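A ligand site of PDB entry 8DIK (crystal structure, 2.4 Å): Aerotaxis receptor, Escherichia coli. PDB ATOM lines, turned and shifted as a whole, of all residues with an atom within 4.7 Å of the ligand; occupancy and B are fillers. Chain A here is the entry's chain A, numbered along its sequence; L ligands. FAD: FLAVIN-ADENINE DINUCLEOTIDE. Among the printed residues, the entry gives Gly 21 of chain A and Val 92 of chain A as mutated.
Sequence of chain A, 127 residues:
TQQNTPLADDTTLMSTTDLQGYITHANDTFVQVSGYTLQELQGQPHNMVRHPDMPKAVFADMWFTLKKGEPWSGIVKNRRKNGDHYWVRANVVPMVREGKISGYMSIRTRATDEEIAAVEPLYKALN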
ATOM      1  N   SER A  15      28.432 -36.622 -32.573  1.00  0.00           N
ATOM      2  CA  SER A  15      27.307 -35.738 -32.852  1.00  0.00           C
ATOM      3  C   SER A  15      27.833 -34.339 -33.114  1.00  0.00           C
ATOM      4  O   SER A  15      28.996 -34.023 -32.855  1.00  0.00           O
ATOM      5  CB  SER A  15      26.295 -35.733 -31.692  1.00  0.00           C
ATOM      6  OG  SER A  15      26.785 -34.993 -30.593  1.00  0.00           O
ATOM      7  N   THR A  17      26.439 -30.138 -32.708  1.00  0.00           N
ATOM      8  CA  THR A  17      25.473 -29.168 -32.233  1.00  0.00           C
ATOM      9  C   THR A  17      25.803 -27.790 -32.780  1.00  0.00           C
ATOM     10  O   THR A  17      26.879 -27.561 -33.338  1.00  0.00           O
ATOM     11  CB  THR A  17      25.425 -29.123 -30.697  1.00  0.00           C
ATOM     12  OG1 THR A  17      26.673 -28.643 -30.198  1.00  0.00           O
ATOM     13  CG2 THR A  17      25.158 -30.511 -30.127  1.00  0.00           C
ATOM     14  N   GLN A  20      24.296 -22.997 -29.619  1.00  0.00           N
ATOM     15  CA  GLN A  20      23.467 -23.039 -28.418  1.00  0.00           C
ATOM     16  C   GLN A  20      23.321 -24.437 -27.846  1.00  0.00           C
ATOM     17  O   GLN A  20      22.597 -24.622 -26.859  1.00  0.00           O
ATOM     18  CB  GLN A  20      22.085 -22.441 -28.691  1.00  0.00           C
ATOM     19  CG  GLN A  20      22.093 -20.960 -29.009  1.00  0.00           C
ATOM     20  CD  GLN A  20      22.365 -20.666 -30.474  1.00  0.00           C
ATOM     21  OE1 GLN A  20      22.209 -21.541 -31.329  1.00  0.00           O
ATOM     22  NE2 GLN A  20      22.774 -19.441 -30.770  1.00  0.00           N
ATOM     23  N   GLY A  21      23.981 -25.441 -28.438  1.00  0.00           N
ATOM     24  CA  GLY A  21      23.924 -26.790 -27.934  1.00  0.00           C
ATOM     25  C   GLY A  21      22.850 -27.666 -28.518  1.00  0.00           C
ATOM     26  O   GLY A  21      22.662 -28.795 -28.042  1.00  0.00           O
ATOM     27  N   HIS A  46      21.327 -31.078 -26.380  1.00  0.00           N
ATOM     28  CA  HIS A  46      22.039 -32.297 -26.007  1.00  0.00           C
ATOM     29  C   HIS A  46      21.815 -32.699 -24.546  1.00  0.00           C
ATOM     30  O   HIS A  46      22.551 -33.545 -24.032  1.00  0.00           O
ATOM     31  CB  HIS A  46      23.540 -32.114 -26.263  1.00  0.00           C
ATOM     32  CG  HIS A  46      24.190 -33.297 -26.916  1.00  0.00           C
ATOM     33  ND1 HIS A  46      24.170 -34.556 -26.367  1.00  0.00           N
ATOM     34  CD2 HIS A  46      24.886 -33.398 -28.073  1.00  0.00           C
ATOM     35  CE1 HIS A  46      24.822 -35.389 -27.152  1.00  0.00           C
ATOM     36  NE2 HIS A  46      25.260 -34.719 -28.200  1.00  0.00           N
ATOM     37  N   ASN A  47      20.819 -32.124 -23.882  1.00  0.00           N
ATOM     38  CA  ASN A  47      20.508 -32.476 -22.502  1.00  0.00           C
ATOM     39  C   ASN A  47      19.437 -33.567 -22.393  1.00  0.00           C
ATOM     40  O   ASN A  47      19.272 -34.128 -21.312  1.00  0.00           O
ATOM     41  CB  ASN A  47      20.067 -31.246 -21.708  1.00  0.00           C
ATOM     42  CG  ASN A  47      18.961 -30.464 -22.403  1.00  0.00           C
ATOM     43  OD1 ASN A  47      18.062 -31.041 -23.013  1.00  0.00           O
ATOM     44  ND2 ASN A  47      19.033 -29.134 -22.302  1.00  0.00           N
ATOM     45  N   VAL A  49      19.921 -36.296 -23.560  1.00  0.00           N
ATOM     46  CA  VAL A  49      20.795 -37.423 -23.266  1.00  0.00           C
ATOM     47  C   VAL A  49      21.343 -37.354 -21.848  1.00  0.00           C
ATOM     48  O   VAL A  49      21.806 -38.380 -21.319  1.00  0.00           O
ATOM     49  CB  VAL A  49      21.956 -37.476 -24.274  1.00  0.00           C
ATOM     50  CG1 VAL A  49      22.694 -38.809 -24.191  1.00  0.00           C
ATOM     51  CG2 VAL A  49      21.445 -37.247 -25.684  1.00  0.00           C
ATOM     52  N   ARG A  50      21.311 -36.184 -21.203  1.00  0.00           N
ATOM     53  CA  ARG A  50      21.935 -36.015 -19.903  1.00  0.00           C
ATOM     54  C   ARG A  50      21.246 -36.855 -18.836  1.00  0.00           C
ATOM     55  O   ARG A  50      20.024 -36.846 -18.712  1.00  0.00           O
ATOM     56  CB  ARG A  50      21.917 -34.540 -19.487  1.00  0.00           C
ATOM     57  CG  ARG A  50      22.096 -34.336 -17.984  1.00  0.00           C
ATOM     58  CD  ARG A  50      22.124 -32.871 -17.594  1.00  0.00           C
ATOM     59  NE  ARG A  50      22.289 -32.721 -16.148  1.00  0.00           N
ATOM     60  CZ  ARG A  50      22.515 -31.560 -15.536  1.00  0.00           C
ATOM     61  NH1 ARG A  50      22.608 -30.438 -16.244  1.00  0.00           N
ATOM     62  NH2 ARG A  50      22.639 -31.520 -14.215  1.00  0.00           N
ATOM     63  N   LYS A  56      25.968 -30.026 -12.254  1.00  0.00           N
ATOM     64  CA  LYS A  56      25.924 -28.824 -13.061  1.00  0.00           C
ATOM     65  C   LYS A  56      27.304 -28.240 -13.284  1.00  0.00           C
ATOM     66  O   LYS A  56      27.545 -27.565 -14.290  1.00  0.00           O
ATOM     67  CB  LYS A  56      25.013 -27.783 -12.404  1.00  0.00           C
ATOM     68  CG  LYS A  56      23.541 -28.171 -12.344  1.00  0.00           C
ATOM     69  CD  LYS A  56      22.680 -26.975 -11.970  1.00  0.00           C
ATOM     70  CE  LYS A  56      21.462 -27.393 -11.178  1.00  0.00           C
ATOM     71  NZ  LYS A  56      20.471 -26.290 -11.061  1.00  0.00           N
ATOM     72  N   PHE A  59      29.157 -29.289 -16.721  1.00  0.00           N
ATOM     73  CA  PHE A  59      28.775 -28.616 -17.952  1.00  0.00           C
ATOM     74  C   PHE A  59      29.091 -27.125 -17.908  1.00  0.00           C
ATOM     75  O   PHE A  59      29.306 -26.511 -18.968  1.00  0.00           O
ATOM     76  CB  PHE A  59      27.284 -28.836 -18.229  1.00  0.00           C
ATOM     77  CG  PHE A  59      26.868 -30.271 -18.164  1.00  0.00           C
ATOM     78  CD1 PHE A  59      27.239 -31.155 -19.171  1.00  0.00           C
ATOM     79  CD2 PHE A  59      26.099 -30.737 -17.116  1.00  0.00           C
ATOM     80  CE1 PHE A  59      26.855 -32.482 -19.115  1.00  0.00           C
ATOM     81  CE2 PHE A  59      25.715 -32.065 -17.060  1.00  0.00           C
ATOM     82  CZ  PHE A  59      26.098 -32.937 -18.061  1.00  0.00           C
ATOM     83  N   ALA A  60      29.111 -26.519 -16.719  1.00  0.00           N
ATOM     84  CA  ALA A  60      29.465 -25.111 -16.621  1.00  0.00           C
ATOM     85  C   ALA A  60      30.936 -24.887 -16.976  1.00  0.00           C
ATOM     86  O   ALA A  60      31.277 -23.864 -17.578  1.00  0.00           O
ATOM     87  CB  ALA A  60      29.171 -24.591 -15.213  1.00  0.00           C
ATOM     88  N   MET A  62      32.610 -26.888 -19.032  1.00  0.00           N
ATOM     89  CA  MET A  62      32.763 -27.213 -20.450  1.00  0.00           C
ATOM     90  C   MET A  62      32.488 -25.997 -21.324  1.00  0.00           C
ATOM     91  O   MET A  62      33.284 -25.670 -22.211  1.00  0.00           O
ATOM     92  CB  MET A  62      31.840 -28.370 -20.819  1.00  0.00           C
ATOM     93  CG  MET A  62      31.916 -28.773 -22.290  1.00  0.00           C
ATOM     94  SD  MET A  62      30.677 -29.997 -22.746  1.00  0.00           S
ATOM     95  CE  MET A  62      29.215 -28.973 -22.864  1.00  0.00           C
ATOM     96  N   TRP A  63      31.349 -25.329 -21.094  1.00  0.00           N
ATOM     97  CA  TRP A  63      31.015 -24.165 -21.905  1.00  0.00           C
ATOM     98  C   TRP A  63      31.945 -22.994 -21.644  1.00  0.00           C
ATOM     99  O   TRP A  63      32.188 -22.177 -22.536  1.00  0.00           O
ATOM    100  CB  TRP A  63      29.561 -23.768 -21.663  1.00  0.00           C
ATOM    101  CG  TRP A  63      28.569 -24.715 -22.255  1.00  0.00           C
ATOM    102  CD1 TRP A  63      27.930 -25.734 -21.613  1.00  0.00           C
ATOM    103  CD2 TRP A  63      28.125 -24.748 -23.617  1.00  0.00           C
ATOM    104  NE1 TRP A  63      27.103 -26.404 -22.494  1.00  0.00           N
ATOM    105  CE2 TRP A  63      27.209 -25.813 -23.728  1.00  0.00           C
ATOM    106  CE3 TRP A  63      28.408 -23.994 -24.752  1.00  0.00           C
ATOM    107  CZ2 TRP A  63      26.571 -26.132 -24.929  1.00  0.00           C
ATOM    108  CZ3 TRP A  63      27.774 -24.299 -25.936  1.00  0.00           C
ATOM    109  CH2 TRP A  63      26.872 -25.367 -26.017  1.00  0.00           C
ATOM    110  N   LEU A  66      34.732 -24.043 -23.816  1.00  0.00           N
ATOM    111  CA  LEU A  66      34.351 -24.001 -25.226  1.00  0.00           C
ATOM    112  C   LEU A  66      34.206 -22.561 -25.726  1.00  0.00           C
ATOM    113  O   LEU A  66      34.598 -22.259 -26.860  1.00  0.00           O
ATOM    114  CB  LEU A  66      33.048 -24.769 -25.442  1.00  0.00           C
ATOM    115  CG  LEU A  66      33.130 -26.289 -25.381  1.00  0.00           C
ATOM    116  CD1 LEU A  66      31.746 -26.906 -25.513  1.00  0.00           C
ATOM    117  CD2 LEU A  66      34.062 -26.831 -26.446  1.00  0.00           C
ATOM    118  N   LYS A  67      33.658 -21.675 -24.898  1.00  0.00           N
ATOM    119  CA  LYS A  67      33.511 -20.284 -25.304  1.00  0.00           C
ATOM    120  C   LYS A  67      34.841 -19.554 -25.364  1.00  0.00           C
ATOM    121  O   LYS A  67      34.929 -18.494 -25.984  1.00  0.00           O
ATOM    122  CB  LYS A  67      32.554 -19.552 -24.360  1.00  0.00           C
ATOM    123  CG  LYS A  67      31.085 -19.890 -24.604  1.00  0.00           C
ATOM    124  CD  LYS A  67      30.160 -19.115 -23.686  1.00  0.00           C
ATOM    125  CE  LYS A  67      28.706 -19.410 -24.005  1.00  0.00           C
ATOM    126  NZ  LYS A  67      27.773 -18.705 -23.080  1.00  0.00           N
ATOM    127  N   VAL A  76      31.492 -38.472 -18.619  1.00  0.00           N
ATOM    128  CA  VAL A  76      30.089 -38.052 -18.610  1.00  0.00           C
ATOM    129  C   VAL A  76      29.206 -39.276 -18.430  1.00  0.00           C
ATOM    130  O   VAL A  76      29.488 -40.350 -18.973  1.00  0.00           O
ATOM    131  CB  VAL A  76      29.726 -37.304 -19.913  1.00  0.00           C
ATOM    132  CG1 VAL A  76      28.320 -36.733 -19.834  1.00  0.00           C
ATOM    133  CG2 VAL A  76      30.739 -36.213 -20.210  1.00  0.00           C
ATOM    134  N   ASN A  78      25.392 -40.558 -19.129  1.00  0.00           N
ATOM    135  CA  ASN A  78      24.285 -40.227 -20.024  1.00  0.00           C
ATOM    136  C   ASN A  78      23.082 -41.117 -19.730  1.00  0.00           C
ATOM    137  O   ASN A  78      23.120 -42.007 -18.869  1.00  0.00           O
ATOM    138  CB  ASN A  78      24.728 -40.371 -21.491  1.00  0.00           C
ATOM    139  CG  ASN A  78      25.694 -39.273 -21.906  1.00  0.00           C
ATOM    140  OD1 ASN A  78      25.691 -38.187 -21.341  1.00  0.00           O
ATOM    141  ND2 ASN A  78      26.522 -39.574 -22.904  1.00  0.00           N
ATOM    142  N   VAL A  92      34.638 -32.764 -26.787  1.00  0.00           N
ATOM    143  CA  VAL A  92      33.982 -31.677 -27.514  1.00  0.00           C
ATOM    144  C   VAL A  92      35.028 -30.683 -27.992  1.00  0.00           C
ATOM    145  O   VAL A  92      35.833 -30.186 -27.193  1.00  0.00           O
ATOM    146  CB  VAL A  92      32.930 -30.991 -26.627  1.00  0.00           C
ATOM    147  CG1 VAL A  92      32.128 -29.986 -27.446  1.00  0.00           C
ATOM    148  CG2 VAL A  92      32.016 -32.017 -25.978  1.00  0.00           C
ATOM    149  N   TYR A 104      30.290 -26.904 -32.376  1.00  0.00           N
ATOM    150  CA  TYR A 104      31.083 -27.847 -31.601  1.00  0.00           C
ATOM    151  C   TYR A 104      30.770 -29.268 -32.035  1.00  0.00           C
ATOM    152  O   TYR A 104      29.594 -29.651 -32.111  1.00  0.00           O
ATOM    153  CB  TYR A 104      30.820 -27.688 -30.095  1.00  0.00           C
ATOM    154  CG  TYR A 104      30.700 -26.257 -29.641  1.00  0.00           C
ATOM    155  CD1 TYR A 104      31.827 -25.500 -29.361  1.00  0.00           C
ATOM    156  CD2 TYR A 104      29.451 -25.651 -29.492  1.00  0.00           C
ATOM    157  CE1 TYR A 104      31.719 -24.182 -28.945  1.00  0.00           C
ATOM    158  CE2 TYR A 104      29.341 -24.343 -29.074  1.00  0.00           C
ATOM    159  CZ  TYR A 104      30.475 -23.609 -28.801  1.00  0.00           C
ATOM    160  OH  TYR A 104      30.364 -22.303 -28.392  1.00  0.00           O
ATOM    161  N   MET A 105      31.817 -30.034 -32.321  1.00  0.00           N
ATOM    162  CA  MET A 105      31.707 -31.458 -32.613  1.00  0.00           C
ATOM    163  C   MET A 105      32.291 -32.246 -31.442  1.00  0.00           C
ATOM    164  O   MET A 105      33.173 -31.765 -30.725  1.00  0.00           O
ATOM    165  CB  MET A 105      32.445 -31.812 -33.906  1.00  0.00           C
ATOM    166  CG  MET A 105      32.088 -33.180 -34.480  1.00  0.00           C
ATOM    167  SD  MET A 105      32.903 -33.486 -36.057  1.00  0.00           S
ATOM    168  CE  MET A 105      32.285 -32.111 -37.034  1.00  0.00           C
ATOM    169  N   SER A 106      31.787 -33.467 -31.244  1.00  0.00           N
ATOM    170  CA  SER A 106      32.228 -34.284 -30.115  1.00  0.00           C
ATOM    171  C   SER A 106      32.279 -35.751 -30.528  1.00  0.00           C
ATOM    172  O   SER A 106      31.404 -36.235 -31.256  1.00  0.00           O
ATOM    173  CB  SER A 106      31.304 -34.109 -28.905  1.00  0.00           C
ATOM    174  OG  SER A 106      31.351 -35.251 -28.061  1.00  0.00           O
ATOM    175  N   ARG A 108      32.562 -39.392 -28.585  1.00  0.00           N
ATOM    176  CA  ARG A 108      32.398 -39.986 -27.257  1.00  0.00           C
ATOM    177  C   ARG A 108      32.667 -41.482 -27.327  1.00  0.00           C
ATOM    178  O   ARG A 108      31.898 -42.228 -27.951  1.00  0.00           O
ATOM    179  CB  ARG A 108      30.995 -39.704 -26.707  1.00  0.00           C
ATOM    180  CG  ARG A 108      30.671 -38.230 -26.571  1.00  0.00           C
ATOM    181  CD  ARG A 108      29.194 -38.020 -26.262  1.00  0.00           C
ATOM    182  NE  ARG A 108      28.339 -38.527 -27.331  1.00  0.00           N
ATOM    183  CZ  ARG A 108      27.894 -37.785 -28.349  1.00  0.00           C
ATOM    184  NH1 ARG A 108      28.218 -36.502 -28.436  1.00  0.00           N
ATOM    185  NH2 ARG A 108      27.116 -38.336 -29.276  1.00  0.00           N
HETATM  186  PA  FAD L   1      22.473 -26.932 -16.903  1.00  0.00           P
HETATM  187  O1A FAD L   1      21.851 -26.663 -15.579  1.00  0.00           O
HETATM  188  O2A FAD L   1      22.108 -25.939 -18.002  1.00  0.00           O
HETATM  189  O5B FAD L   1      24.040 -26.984 -16.785  1.00  0.00           O
HETATM  190  C5B FAD L   1      24.742 -26.338 -15.701  1.00  0.00           C
HETATM  191  C4B FAD L   1      25.553 -25.186 -16.247  1.00  0.00           C
HETATM  192  O4B FAD L   1      25.865 -25.422 -17.629  1.00  0.00           O
HETATM  193  C3B FAD L   1      24.858 -23.830 -16.260  1.00  0.00           C
HETATM  194  O3B FAD L   1      24.964 -23.200 -14.986  1.00  0.00           O
HETATM  195  C2B FAD L   1      25.637 -23.074 -17.344  1.00  0.00           C
HETATM  196  O2B FAD L   1      26.695 -22.295 -16.787  1.00  0.00           O
HETATM  197  C1B FAD L   1      26.199 -24.193 -18.236  1.00  0.00           C
HETATM  198  N9A FAD L   1      25.679 -24.179 -19.596  1.00  0.00           N
HETATM  199  C8A FAD L   1      24.908 -25.138 -20.202  1.00  0.00           C
HETATM  200  N7A FAD L   1      24.598 -24.866 -21.448  1.00  0.00           N
HETATM  201  C5A FAD L   1      25.208 -23.643 -21.685  1.00  0.00           C
HETATM  202  C6A FAD L   1      25.268 -22.805 -22.811  1.00  0.00           C
HETATM  203  N6A FAD L   1      24.670 -23.088 -23.975  1.00  0.00           N
HETATM  204  N1A FAD L   1      25.969 -21.654 -22.714  1.00  0.00           N
HETATM  205  C2A FAD L   1      26.567 -21.371 -21.550  1.00  0.00           C
HETATM  206  N3A FAD L   1      26.583 -22.081 -20.425  1.00  0.00           N
HETATM  207  C4A FAD L   1      25.882 -23.208 -20.548  1.00  0.00           C
HETATM  208  N1  FAD L   1      25.600 -33.262 -22.310  1.00  0.00           N
HETATM  209  C2  FAD L   1      25.405 -34.548 -21.891  1.00  0.00           C
HETATM  210  O2  FAD L   1      24.868 -34.810 -20.814  1.00  0.00           O
HETATM  211  N3  FAD L   1      25.825 -35.595 -22.702  1.00  0.00           N
HETATM  212  C4  FAD L   1      26.436 -35.478 -23.925  1.00  0.00           C
HETATM  213  O4  FAD L   1      26.764 -36.493 -24.551  1.00  0.00           O
HETATM  214  C4X FAD L   1      26.639 -34.112 -24.353  1.00  0.00           C
HETATM  215  N5  FAD L   1      27.210 -33.902 -25.507  1.00  0.00           N
HETATM  216  C5X FAD L   1      27.398 -32.594 -25.920  1.00  0.00           C
HETATM  217  C6  FAD L   1      28.011 -32.364 -27.148  1.00  0.00           C
HETATM  218  C7  FAD L   1      28.223 -31.058 -27.606  1.00  0.00           C
HETATM  219  C7M FAD L   1      28.882 -30.846 -28.931  1.00  0.00           C
HETATM  220  C8  FAD L   1      27.805 -29.974 -26.814  1.00  0.00           C
HETATM  221  C8M FAD L   1      28.019 -28.556 -27.277  1.00  0.00           C
HETATM  222  C9  FAD L   1      27.201 -30.205 -25.587  1.00  0.00           C
HETATM  223  C9A FAD L   1      26.989 -31.504 -25.141  1.00  0.00           C
HETATM  224  N10 FAD L   1      26.373 -31.779 -23.892  1.00  0.00           N
HETATM  225  C10 FAD L   1      26.178 -33.065 -23.473  1.00  0.00           C
HETATM  226  C1' FAD L   1      25.927 -30.676 -23.027  1.00  0.00           C
HETATM  227  C2' FAD L   1      24.483 -30.266 -23.289  1.00  0.00           C
HETATM  228  O2' FAD L   1      24.407 -29.425 -24.444  1.00  0.00           O
HETATM  229  C3' FAD L   1      23.944 -29.506 -22.080  1.00  0.00           C
HETATM  230  O3' FAD L   1      24.618 -28.256 -21.970  1.00  0.00           O
HETATM  231  C4' FAD L   1      24.085 -30.261 -20.758  1.00  0.00           C
HETATM  232  O4' FAD L   1      23.270 -31.428 -20.790  1.00  0.00           O
HETATM  233  C5' FAD L   1      23.740 -29.404 -19.553  1.00  0.00           C
HETATM  234  O5' FAD L   1      22.480 -28.740 -19.810  1.00  0.00           O
HETATM  235  P   FAD L   1      21.331 -28.755 -18.737  1.00  0.00           P
HETATM  236  O1P FAD L   1      20.302 -27.653 -19.019  1.00  0.00           O
HETATM  237  O2P FAD L   1      20.747 -30.115 -18.629  1.00  0.00           O
HETATM  238  O3P FAD L   1      22.097 -28.391 -17.391  1.00  0.00           O
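Merely in contact with the ligand: Thr 17, Asn 47, Arg 108, Lys 56, Tyr 104, Phe 59, Ala 60, Met 62, Val 92, Gln 20 and Val 76.
Hydrophobic or aromatic side chains within 4 Å of the ligand: His 46, Phe 59, Ala 60, Met 62, Trp 63, Val 76, Val 92 and Tyr 104.
The nearest printed residue that does not touch the ligand is Gly 21 (4.05 Å).
NE2 of His 46 sits at hydrogen-bond distance from NH1 of Arg 108, at 3.5 Å.
The backbone NH (N) of His 46 lies within hydrogen-bond range of the backbone carbonyl oxygen (O) of Gly 21 (3.1 Å).
NE2 of His 46 lies within hydrogen-bond range of OG of Ser 15 (2.9 Å).
The backbone carbonyl oxygen (O) of Tyr 104 is in hydrogen-bond range of the backbone NH (N) of Thr 17, 3.2 Å away.
The side-chain hydroxyl (OG) of Ser 106 lies within hydrogen-bond range of the guanidinium group (NH1) of Arg 108, at 3.4 Å.
OG of Ser 15 lies within hydrogen-bond range of NH1 of Arg 108 (3.0 Å).
O2P of the ligand is in salt-bridge range of NH1 of Arg 50 (3.0 Å).
A nitrogen (N3) of the ligand lies within hydrogen-bond range of the side-chain amide oxygen (OD1) of Asn 78, at 2.9 Å.
A nitrogen (N7A) of the ligand lies within hydrogen-bond range of the indole nitrogen (NE1) of Trp 63, at 3.1 Å.
ND1 of His 46 sits close to N5 of the ligand, at 3.2 Å.
NZ of Lys 67 sits close to N1A of the ligand (3.5 Å).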
